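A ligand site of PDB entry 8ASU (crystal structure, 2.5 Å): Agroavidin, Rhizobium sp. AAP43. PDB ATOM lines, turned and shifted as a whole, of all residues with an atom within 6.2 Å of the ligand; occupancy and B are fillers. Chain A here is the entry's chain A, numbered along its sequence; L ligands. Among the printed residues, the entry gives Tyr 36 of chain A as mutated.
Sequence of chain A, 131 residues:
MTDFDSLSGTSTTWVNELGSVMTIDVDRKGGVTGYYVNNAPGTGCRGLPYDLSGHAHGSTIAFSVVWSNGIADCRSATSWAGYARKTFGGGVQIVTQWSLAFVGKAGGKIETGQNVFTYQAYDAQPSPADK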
ATOM      1  N   ASN A  16       3.868  -9.631 -11.863  1.00  0.00           N
ATOM      2  CA  ASN A  16       3.687 -11.100 -12.011  1.00  0.00           C
ATOM      3  C   ASN A  16       2.903 -11.326 -13.319  1.00  0.00           C
ATOM      4  O   ASN A  16       2.469 -10.303 -13.912  1.00  0.00           O
ATOM      5  CB  ASN A  16       3.123 -11.755 -10.749  1.00  0.00           C
ATOM      6  CG  ASN A  16       1.677 -11.413 -10.453  1.00  0.00           C
ATOM      7  OD1 ASN A  16       0.955 -10.942 -11.327  1.00  0.00           O
ATOM      8  ND2 ASN A  16       1.269 -11.688  -9.218  1.00  0.00           N
ATOM      9  N   LEU A  18       0.069 -12.514 -13.896  1.00  0.00           N
ATOM     10  CA  LEU A  18      -1.355 -12.099 -13.771  1.00  0.00           C
ATOM     11  C   LEU A  18      -1.493 -10.582 -13.998  1.00  0.00           C
ATOM     12  O   LEU A  18      -2.627 -10.092 -14.021  1.00  0.00           O
ATOM     13  CB  LEU A  18      -1.867 -12.500 -12.383  1.00  0.00           C
ATOM     14  CG  LEU A  18      -1.606 -13.948 -11.973  1.00  0.00           C
ATOM     15  CD1 LEU A  18      -2.199 -14.235 -10.604  1.00  0.00           C
ATOM     16  CD2 LEU A  18      -2.148 -14.917 -13.000  1.00  0.00           C
ATOM     17  N   GLY A  19      -0.372  -9.865 -14.131  1.00  0.00           N
ATOM     18  CA  GLY A  19      -0.303  -8.390 -14.248  1.00  0.00           C
ATOM     19  C   GLY A  19      -0.659  -7.653 -12.954  1.00  0.00           C
ATOM     20  O   GLY A  19      -1.142  -6.481 -13.056  1.00  0.00           O
ATOM     21  N   SER A  20      -0.468  -8.279 -11.787  1.00  0.00           N
ATOM     22  CA  SER A  20      -0.491  -7.585 -10.472  1.00  0.00           C
ATOM     23  C   SER A  20       0.894  -6.948 -10.276  1.00  0.00           C
ATOM     24  O   SER A  20       1.858  -7.426 -10.901  1.00  0.00           O
ATOM     25  CB  SER A  20      -0.861  -8.528  -9.352  1.00  0.00           C
ATOM     26  OG  SER A  20      -2.155  -9.067  -9.547  1.00  0.00           O
ATOM     27  N   VAL A  21       0.968  -5.865  -9.500  1.00  0.00           N
ATOM     28  CA  VAL A  21       2.216  -5.049  -9.365  1.00  0.00           C
ATOM     29  C   VAL A  21       2.500  -4.882  -7.881  1.00  0.00           C
ATOM     30  O   VAL A  21       1.545  -4.833  -7.074  1.00  0.00           O
ATOM     31  CB  VAL A  21       2.100  -3.677 -10.054  1.00  0.00           C
ATOM     32  CG1 VAL A  21       3.452  -3.052 -10.368  1.00  0.00           C
ATOM     33  CG2 VAL A  21       1.261  -3.755 -11.306  1.00  0.00           C
ATOM     34  N   TYR A  36       0.953  -3.542  -2.826  1.00  0.00           N
ATOM     35  CA  TYR A  36       0.553  -4.550  -3.827  1.00  0.00           C
ATOM     36  C   TYR A  36      -0.675  -4.004  -4.522  1.00  0.00           C
ATOM     37  O   TYR A  36      -1.531  -3.402  -3.814  1.00  0.00           O
ATOM     38  CB  TYR A  36       0.277  -5.899  -3.162  1.00  0.00           C
ATOM     39  CG  TYR A  36       0.387  -7.073  -4.100  1.00  0.00           C
ATOM     40  CD1 TYR A  36      -0.676  -7.489  -4.897  1.00  0.00           C
ATOM     41  CD2 TYR A  36       1.569  -7.782  -4.188  1.00  0.00           C
ATOM     42  CE1 TYR A  36      -0.557  -8.584  -5.733  1.00  0.00           C
ATOM     43  CE2 TYR A  36       1.701  -8.880  -5.027  1.00  0.00           C
ATOM     44  CZ  TYR A  36       0.642  -9.283  -5.798  1.00  0.00           C
ATOM     45  OH  TYR A  36       0.819 -10.376  -6.599  1.00  0.00           O
ATOM     46  N   VAL A  37      -0.734  -4.178  -5.849  1.00  0.00           N
ATOM     47  CA  VAL A  37      -1.933  -3.875  -6.668  1.00  0.00           C
ATOM     48  C   VAL A  37      -2.297  -5.150  -7.428  1.00  0.00           C
ATOM     49  O   VAL A  37      -1.666  -5.483  -8.444  1.00  0.00           O
ATOM     50  CB  VAL A  37      -1.749  -2.654  -7.580  1.00  0.00           C
ATOM     51  CG1 VAL A  37      -3.064  -2.231  -8.194  1.00  0.00           C
ATOM     52  CG2 VAL A  37      -1.125  -1.487  -6.822  1.00  0.00           C
ATOM     53  N   ASN A  38      -3.286  -5.853  -6.888  1.00  0.00           N
ATOM     54  CA  ASN A  38      -3.883  -7.034  -7.550  1.00  0.00           C
ATOM     55  C   ASN A  38      -4.560  -6.606  -8.855  1.00  0.00           C
ATOM     56  O   ASN A  38      -5.392  -5.651  -8.815  1.00  0.00           O
ATOM     57  CB  ASN A  38      -4.868  -7.706  -6.611  1.00  0.00           C
ATOM     58  CG  ASN A  38      -5.568  -8.842  -7.296  1.00  0.00           C
ATOM     59  OD1 ASN A  38      -4.935  -9.520  -8.107  1.00  0.00           O
ATOM     60  ND2 ASN A  38      -6.854  -9.020  -7.013  1.00  0.00           N
ATOM     61  N   ASN A  39      -4.222  -7.268  -9.957  1.00  0.00           N
ATOM     62  CA  ASN A  39      -4.910  -7.145 -11.261  1.00  0.00           C
ATOM     63  C   ASN A  39      -5.179  -8.551 -11.796  1.00  0.00           C
ATOM     64  O   ASN A  39      -5.229  -8.745 -13.025  1.00  0.00           O
ATOM     65  CB  ASN A  39      -4.110  -6.296 -12.267  1.00  0.00           C
ATOM     66  CG  ASN A  39      -4.058  -4.829 -11.894  1.00  0.00           C
ATOM     67  OD1 ASN A  39      -5.094  -4.187 -11.723  1.00  0.00           O
ATOM     68  ND2 ASN A  39      -2.861  -4.285 -11.745  1.00  0.00           N
ATOM     69  N   ALA A  40      -5.353  -9.520 -10.888  1.00  0.00           N
ATOM     70  CA  ALA A  40      -5.557 -10.932 -11.256  1.00  0.00           C
ATOM     71  C   ALA A  40      -7.020 -11.134 -11.640  1.00  0.00           C
ATOM     72  O   ALA A  40      -7.911 -10.817 -10.850  1.00  0.00           O
ATOM     73  CB  ALA A  40      -5.149 -11.821 -10.112  1.00  0.00           C
ATOM     74  N   GLY A  42     -10.702 -12.707 -12.183  1.00  0.00           N
ATOM     75  CA  GLY A  42     -11.575 -13.581 -11.385  1.00  0.00           C
ATOM     76  C   GLY A  42     -11.363 -13.377  -9.895  1.00  0.00           C
ATOM     77  O   GLY A  42     -11.904 -14.198  -9.141  1.00  0.00           O
ATOM     78  N   THR A  43     -10.657 -12.324  -9.478  1.00  0.00           N
ATOM     79  CA  THR A  43     -10.373 -12.057  -8.035  1.00  0.00           C
ATOM     80  C   THR A  43     -11.013 -10.731  -7.604  1.00  0.00           C
ATOM     81  O   THR A  43     -11.315  -9.914  -8.467  1.00  0.00           O
ATOM     82  CB  THR A  43      -8.863 -12.115  -7.730  1.00  0.00           C
ATOM     83  OG1 THR A  43      -8.205 -10.991  -8.341  1.00  0.00           O
ATOM     84  CG2 THR A  43      -8.226 -13.401  -8.184  1.00  0.00           C
ATOM     85  N   GLY A  44     -11.186 -10.526  -6.309  1.00  0.00           N
ATOM     86  CA  GLY A  44     -11.673  -9.245  -5.766  1.00  0.00           C
ATOM     87  C   GLY A  44     -10.548  -8.268  -5.487  1.00  0.00           C
ATOM     88  O   GLY A  44      -9.357  -8.601  -5.748  1.00  0.00           O
ATOM     89  N   CYS A  45     -10.904  -7.096  -4.964  1.00  0.00           N
ATOM     90  CA  CYS A  45      -9.963  -6.075  -4.432  1.00  0.00           C
ATOM     91  C   CYS A  45      -8.911  -5.787  -5.514  1.00  0.00           C
ATOM     92  O   CYS A  45      -7.688  -5.831  -5.228  1.00  0.00           O
ATOM     93  CB  CYS A  45      -9.374  -6.570  -3.125  1.00  0.00           C
ATOM     94  SG  CYS A  45     -10.548  -6.598  -1.741  1.00  0.00           S
ATOM     95  N   TRP A  67      -6.278  -8.179   2.377  1.00  0.00           N
ATOM     96  CA  TRP A  67      -7.098  -7.486   1.350  1.00  0.00           C
ATOM     97  C   TRP A  67      -8.132  -6.573   2.015  1.00  0.00           C
ATOM     98  O   TRP A  67      -9.319  -6.687   1.696  1.00  0.00           O
ATOM     99  CB  TRP A  67      -7.723  -8.538   0.457  1.00  0.00           C
ATOM    100  CG  TRP A  67      -6.651  -9.300  -0.246  1.00  0.00           C
ATOM    101  CD1 TRP A  67      -6.232 -10.584  -0.049  1.00  0.00           C
ATOM    102  CD2 TRP A  67      -5.773  -8.722  -1.220  1.00  0.00           C
ATOM    103  NE1 TRP A  67      -5.178 -10.866  -0.868  1.00  0.00           N
ATOM    104  CE2 TRP A  67      -4.869  -9.733  -1.594  1.00  0.00           C
ATOM    105  CE3 TRP A  67      -5.680  -7.460  -1.800  1.00  0.00           C
ATOM    106  CZ2 TRP A  67      -3.882  -9.509  -2.555  1.00  0.00           C
ATOM    107  CZ3 TRP A  67      -4.715  -7.241  -2.752  1.00  0.00           C
ATOM    108  CH2 TRP A  67      -3.821  -8.253  -3.108  1.00  0.00           C
ATOM    109  N   CYS A  74     -11.950  -7.744   0.885  1.00  0.00           N
ATOM    110  CA  CYS A  74     -12.314  -9.087   0.331  1.00  0.00           C
ATOM    111  C   CYS A  74     -12.271 -10.194   1.397  1.00  0.00           C
ATOM    112  O   CYS A  74     -12.430 -11.366   1.021  1.00  0.00           O
ATOM    113  CB  CYS A  74     -11.406  -9.404  -0.845  1.00  0.00           C
ATOM    114  SG  CYS A  74     -11.650  -8.237  -2.214  1.00  0.00           S
ATOM    115  N   ARG A  75     -12.133  -9.841   2.687  1.00  0.00           N
ATOM    116  CA  ARG A  75     -12.154 -10.799   3.827  1.00  0.00           C
ATOM    117  C   ARG A  75     -11.221 -11.970   3.475  1.00  0.00           C
ATOM    118  O   ARG A  75     -11.689 -13.120   3.440  1.00  0.00           O
ATOM    119  CB  ARG A  75     -13.578 -11.288   4.106  1.00  0.00           C
ATOM    120  CG  ARG A  75     -14.494 -10.201   4.662  1.00  0.00           C
ATOM    121  CD  ARG A  75     -15.939 -10.648   4.616  1.00  0.00           C
ATOM    122  NE  ARG A  75     -16.820  -9.511   4.823  1.00  0.00           N
ATOM    123  CZ  ARG A  75     -18.148  -9.580   4.771  1.00  0.00           C
ATOM    124  NH1 ARG A  75     -18.872  -8.485   4.954  1.00  0.00           N
ATOM    125  NH2 ARG A  75     -18.743 -10.731   4.556  1.00  0.00           N
ATOM    126  N   SER A  76      -9.965 -11.646   3.181  1.00  0.00           N
ATOM    127  CA  SER A  76      -8.902 -12.581   2.755  1.00  0.00           C
ATOM    128  C   SER A  76      -7.526 -11.988   3.082  1.00  0.00           C
ATOM    129  O   SER A  76      -7.457 -10.811   3.486  1.00  0.00           O
ATOM    130  CB  SER A  76      -9.045 -12.894   1.289  1.00  0.00           C
ATOM    131  OG  SER A  76      -9.062 -11.704   0.522  1.00  0.00           O
ATOM    132  N   THR A  78      -3.146 -12.901   1.760  1.00  0.00           N
ATOM    133  CA  THR A  78      -2.152 -13.684   0.997  1.00  0.00           C
ATOM    134  C   THR A  78      -0.757 -13.476   1.574  1.00  0.00           C
ATOM    135  O   THR A  78      -0.485 -12.398   2.176  1.00  0.00           O
ATOM    136  CB  THR A  78      -2.206 -13.290  -0.473  1.00  0.00           C
ATOM    137  OG1 THR A  78      -3.586 -13.491  -0.737  1.00  0.00           O
ATOM    138  CG2 THR A  78      -1.297 -14.124  -1.336  1.00  0.00           C
ATOM    139  N   TRP A  80       3.413 -14.753   0.457  1.00  0.00           N
ATOM    140  CA  TRP A  80       4.293 -15.224  -0.638  1.00  0.00           C
ATOM    141  C   TRP A  80       5.634 -15.580   0.018  1.00  0.00           C
ATOM    142  O   TRP A  80       6.052 -14.875   0.968  1.00  0.00           O
ATOM    143  CB  TRP A  80       4.508 -14.120  -1.690  1.00  0.00           C
ATOM    144  CG  TRP A  80       3.354 -13.777  -2.595  1.00  0.00           C
ATOM    145  CD1 TRP A  80       3.160 -14.200  -3.876  1.00  0.00           C
ATOM    146  CD2 TRP A  80       2.315 -12.814  -2.340  1.00  0.00           C
ATOM    147  NE1 TRP A  80       2.056 -13.598  -4.424  1.00  0.00           N
ATOM    148  CE2 TRP A  80       1.514 -12.753  -3.504  1.00  0.00           C
ATOM    149  CE3 TRP A  80       1.962 -12.014  -1.239  1.00  0.00           C
ATOM    150  CZ2 TRP A  80       0.385 -11.939  -3.590  1.00  0.00           C
ATOM    151  CZ3 TRP A  80       0.856 -11.194  -1.335  1.00  0.00           C
ATOM    152  CH2 TRP A  80       0.073 -11.172  -2.502  1.00  0.00           C
ATOM    153  N   TRP A  98       2.442 -18.716  -3.251  1.00  0.00           N
ATOM    154  CA  TRP A  98       1.470 -17.961  -2.418  1.00  0.00           C
ATOM    155  C   TRP A  98       0.426 -18.892  -1.818  1.00  0.00           C
ATOM    156  O   TRP A  98       0.127 -19.940  -2.411  1.00  0.00           O
ATOM    157  CB  TRP A  98       0.822 -16.830  -3.226  1.00  0.00           C
ATOM    158  CG  TRP A  98       0.102 -17.238  -4.482  1.00  0.00           C
ATOM    159  CD1 TRP A  98       0.555 -17.098  -5.767  1.00  0.00           C
ATOM    160  CD2 TRP A  98      -1.224 -17.767  -4.591  1.00  0.00           C
ATOM    161  NE1 TRP A  98      -0.386 -17.524  -6.655  1.00  0.00           N
ATOM    162  CE2 TRP A  98      -1.491 -17.936  -5.972  1.00  0.00           C
ATOM    163  CE3 TRP A  98      -2.212 -18.134  -3.672  1.00  0.00           C
ATOM    164  CZ2 TRP A  98      -2.696 -18.442  -6.450  1.00  0.00           C
ATOM    165  CZ3 TRP A  98      -3.413 -18.631  -4.147  1.00  0.00           C
ATOM    166  CH2 TRP A  98      -3.646 -18.785  -5.507  1.00  0.00           C
ATOM    167  N   LEU A 100      -3.476 -18.124  -0.381  1.00  0.00           N
ATOM    168  CA  LEU A 100      -4.647 -17.253  -0.138  1.00  0.00           C
ATOM    169  C   LEU A 100      -5.564 -17.919   0.889  1.00  0.00           C
ATOM    170  O   LEU A 100      -6.105 -18.984   0.570  1.00  0.00           O
ATOM    171  CB  LEU A 100      -5.350 -17.057  -1.482  1.00  0.00           C
ATOM    172  CG  LEU A 100      -6.700 -16.342  -1.426  1.00  0.00           C
ATOM    173  CD1 LEU A 100      -6.601 -15.076  -0.590  1.00  0.00           C
ATOM    174  CD2 LEU A 100      -7.176 -16.018  -2.825  1.00  0.00           C
ATOM    175  N   PHE A 102      -9.143 -17.316   2.919  1.00  0.00           N
ATOM    176  CA  PHE A 102     -10.428 -16.566   2.958  1.00  0.00           C
ATOM    177  C   PHE A 102     -11.495 -17.336   3.727  1.00  0.00           C
ATOM    178  O   PHE A 102     -11.396 -18.567   3.934  1.00  0.00           O
ATOM    179  CB  PHE A 102     -10.963 -16.285   1.556  1.00  0.00           C
ATOM    180  CG  PHE A 102     -11.342 -17.503   0.767  1.00  0.00           C
ATOM    181  CD1 PHE A 102     -10.375 -18.276   0.128  1.00  0.00           C
ATOM    182  CD2 PHE A 102     -12.673 -17.861   0.605  1.00  0.00           C
ATOM    183  CE1 PHE A 102     -10.723 -19.362  -0.660  1.00  0.00           C
ATOM    184  CE2 PHE A 102     -13.023 -18.974  -0.161  1.00  0.00           C
ATOM    185  CZ  PHE A 102     -12.050 -19.707  -0.795  1.00  0.00           C
ATOM    186  N   ASN A 115       3.316 -17.496  -8.218  1.00  0.00           N
ATOM    187  CA  ASN A 115       3.555 -16.236  -8.991  1.00  0.00           C
ATOM    188  C   ASN A 115       5.065 -16.084  -9.246  1.00  0.00           C
ATOM    189  O   ASN A 115       5.849 -16.315  -8.323  1.00  0.00           O
ATOM    190  CB  ASN A 115       3.050 -14.968  -8.296  1.00  0.00           C
ATOM    191  CG  ASN A 115       1.553 -14.846  -8.206  1.00  0.00           C
ATOM    192  OD1 ASN A 115       1.025 -14.347  -7.213  1.00  0.00           O
ATOM    193  ND2 ASN A 115       0.831 -15.259  -9.241  1.00  0.00           N
ATOM    194  N   PHE A 117       7.572 -12.948 -10.318  1.00  0.00           N
ATOM    195  CA  PHE A 117       7.639 -11.461 -10.354  1.00  0.00           C
ATOM    196  C   PHE A 117       8.887 -11.046 -11.126  1.00  0.00           C
ATOM    197  O   PHE A 117       9.926 -11.684 -10.875  1.00  0.00           O
ATOM    198  CB  PHE A 117       7.704 -10.918  -8.935  1.00  0.00           C
ATOM    199  CG  PHE A 117       6.417 -11.102  -8.186  1.00  0.00           C
ATOM    200  CD1 PHE A 117       5.399 -10.188  -8.305  1.00  0.00           C
ATOM    201  CD2 PHE A 117       6.233 -12.200  -7.360  1.00  0.00           C
ATOM    202  CE1 PHE A 117       4.219 -10.370  -7.632  1.00  0.00           C
ATOM    203  CE2 PHE A 117       5.046 -12.373  -6.667  1.00  0.00           C
ATOM    204  CZ  PHE A 117       4.030 -11.458  -6.832  1.00  0.00           C
HETATM  205  C1  LIG L   1      -9.404 -11.751  -3.195  1.00  0.00           C
HETATM  206  O1  LIG L   1      -9.719 -12.034  -4.377  1.00  0.00           O
HETATM  207  O2  LIG L   1      -9.972 -12.218  -2.170  1.00  0.00           O
HETATM  208  C2  LIG L   1      -8.278 -10.774  -2.915  1.00  0.00           C
HETATM  209  C3  LIG L   1      -7.242 -10.678  -4.040  1.00  0.00           C
HETATM  210  C4  LIG L   1      -6.349 -11.915  -4.140  1.00  0.00           C
HETATM  211  C5  LIG L   1      -5.417 -11.848  -5.376  1.00  0.00           C
HETATM  212  C6  LIG L   1      -4.496 -13.059  -5.411  1.00  0.00           C
HETATM  213  S1  LIG L   1      -3.171 -12.940  -4.216  1.00  0.00           S
HETATM  214  C7  LIG L   1      -2.476 -14.354  -5.003  1.00  0.00           C
HETATM  215  C8  LIG L   1      -2.603 -14.151  -6.480  1.00  0.00           C
HETATM  216  N1  LIG L   1      -1.548 -13.311  -7.008  1.00  0.00           N
HETATM  217  C9  LIG L   1      -2.009 -12.153  -7.493  1.00  0.00           C
HETATM  218  O3  LIG L   1      -1.339 -11.255  -7.980  1.00  0.00           O
HETATM  219  N2  LIG L   1      -3.324 -12.127  -7.345  1.00  0.00           N
HETATM  220  C10 LIG L   1      -3.838 -13.325  -6.745  1.00  0.00           C
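An oxygen (O3) of the ligand is in hydrogen-bond range of the side-chain hydroxyl (OH) of Tyr 36 (2.7 Å). A nitrogen (N1) of the ligand sits at hydrogen-bond distance from the side-chain amide oxygen of Asn 115. The side-chain hydroxyl (OG) of Ser 20 is in hydrogen-bond range of an oxygen (O3) of the ligand, at 2.8 Å. N of Gly 44 sits at hydrogen-bond distance from O1 of the ligand. An oxygen (O2) of the ligand sits at hydrogen-bond distance from the side-chain hydroxyl (OG) of Ser 76. The side-chain amide nitrogen (ND2) of Asn 16 is in hydrogen-bond range of an oxygen (O3) of the ligand (2.9 Å). OD1 of Asn 38 sits at hydrogen-bond distance from N2 of the ligand. S1 of the ligand sits close to OG1 of Thr 78.
OH of Tyr 36 is in hydrogen-bond range of ND2 of Asn 16, at 3.0 Å. The side-chain amide nitrogen (ND2) of Asn 16 sits close to the side-chain amide oxygen (OD1) of Asn 115, 3.3 Å away. The backbone NH (N) of Ser 20 is in hydrogen-bond range of the side-chain amide oxygen (OD1) of Asn 16 (3.1 Å). N of Asn 39 lies within hydrogen-bond range of OG of Ser 20. OG of Ser 76 lies within hydrogen-bond range of O of Cys 74, 3.4 Å away. O of Ser 76 is in hydrogen-bond range of N of Trp 67, at 3.1 Å. The side-chain amide oxygen (OD1) of Asn 38 sits at hydrogen-bond distance from the backbone NH (N) of Ala 40 (2.8 Å). OG1 of Thr 78 lies within hydrogen-bond range of NE1 of Trp 67, 3.1 Å away.
CD1 of Leu 18 touches C9 of the ligand, at 3.7 Å. Ala 40 touches the ligand (CB to N2, 3.3 Å). CB of Thr 43 touches O1 of the ligand, 3.5 Å away. Trp 67 touches the ligand. CB of Cys 74 touches O2 of the ligand, at 3.4 Å. Trp 80 touches the ligand (CZ2 to S1, 3.7 Å). Trp 98 touches the ligand (CD2 to C7, 3.7 Å). Hydrophobic or aromatic side chains that line the ligand: Leu 18, Tyr 36, Ala 40, Trp 67, Trp 80 and Trp 98. 15 residues have an atom within 4 Å of the ligand: Asn 16, Leu 18, Ser 20, Tyr 36, Asn 38, Ala 40, Thr 43, Gly 44, Trp 67, Cys 74, Ser 76, Thr 78, Trp 80, Trp 98 and Asn 115. The nearest printed residue that does not touch the ligand is Cys 45 (4.3 Å).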
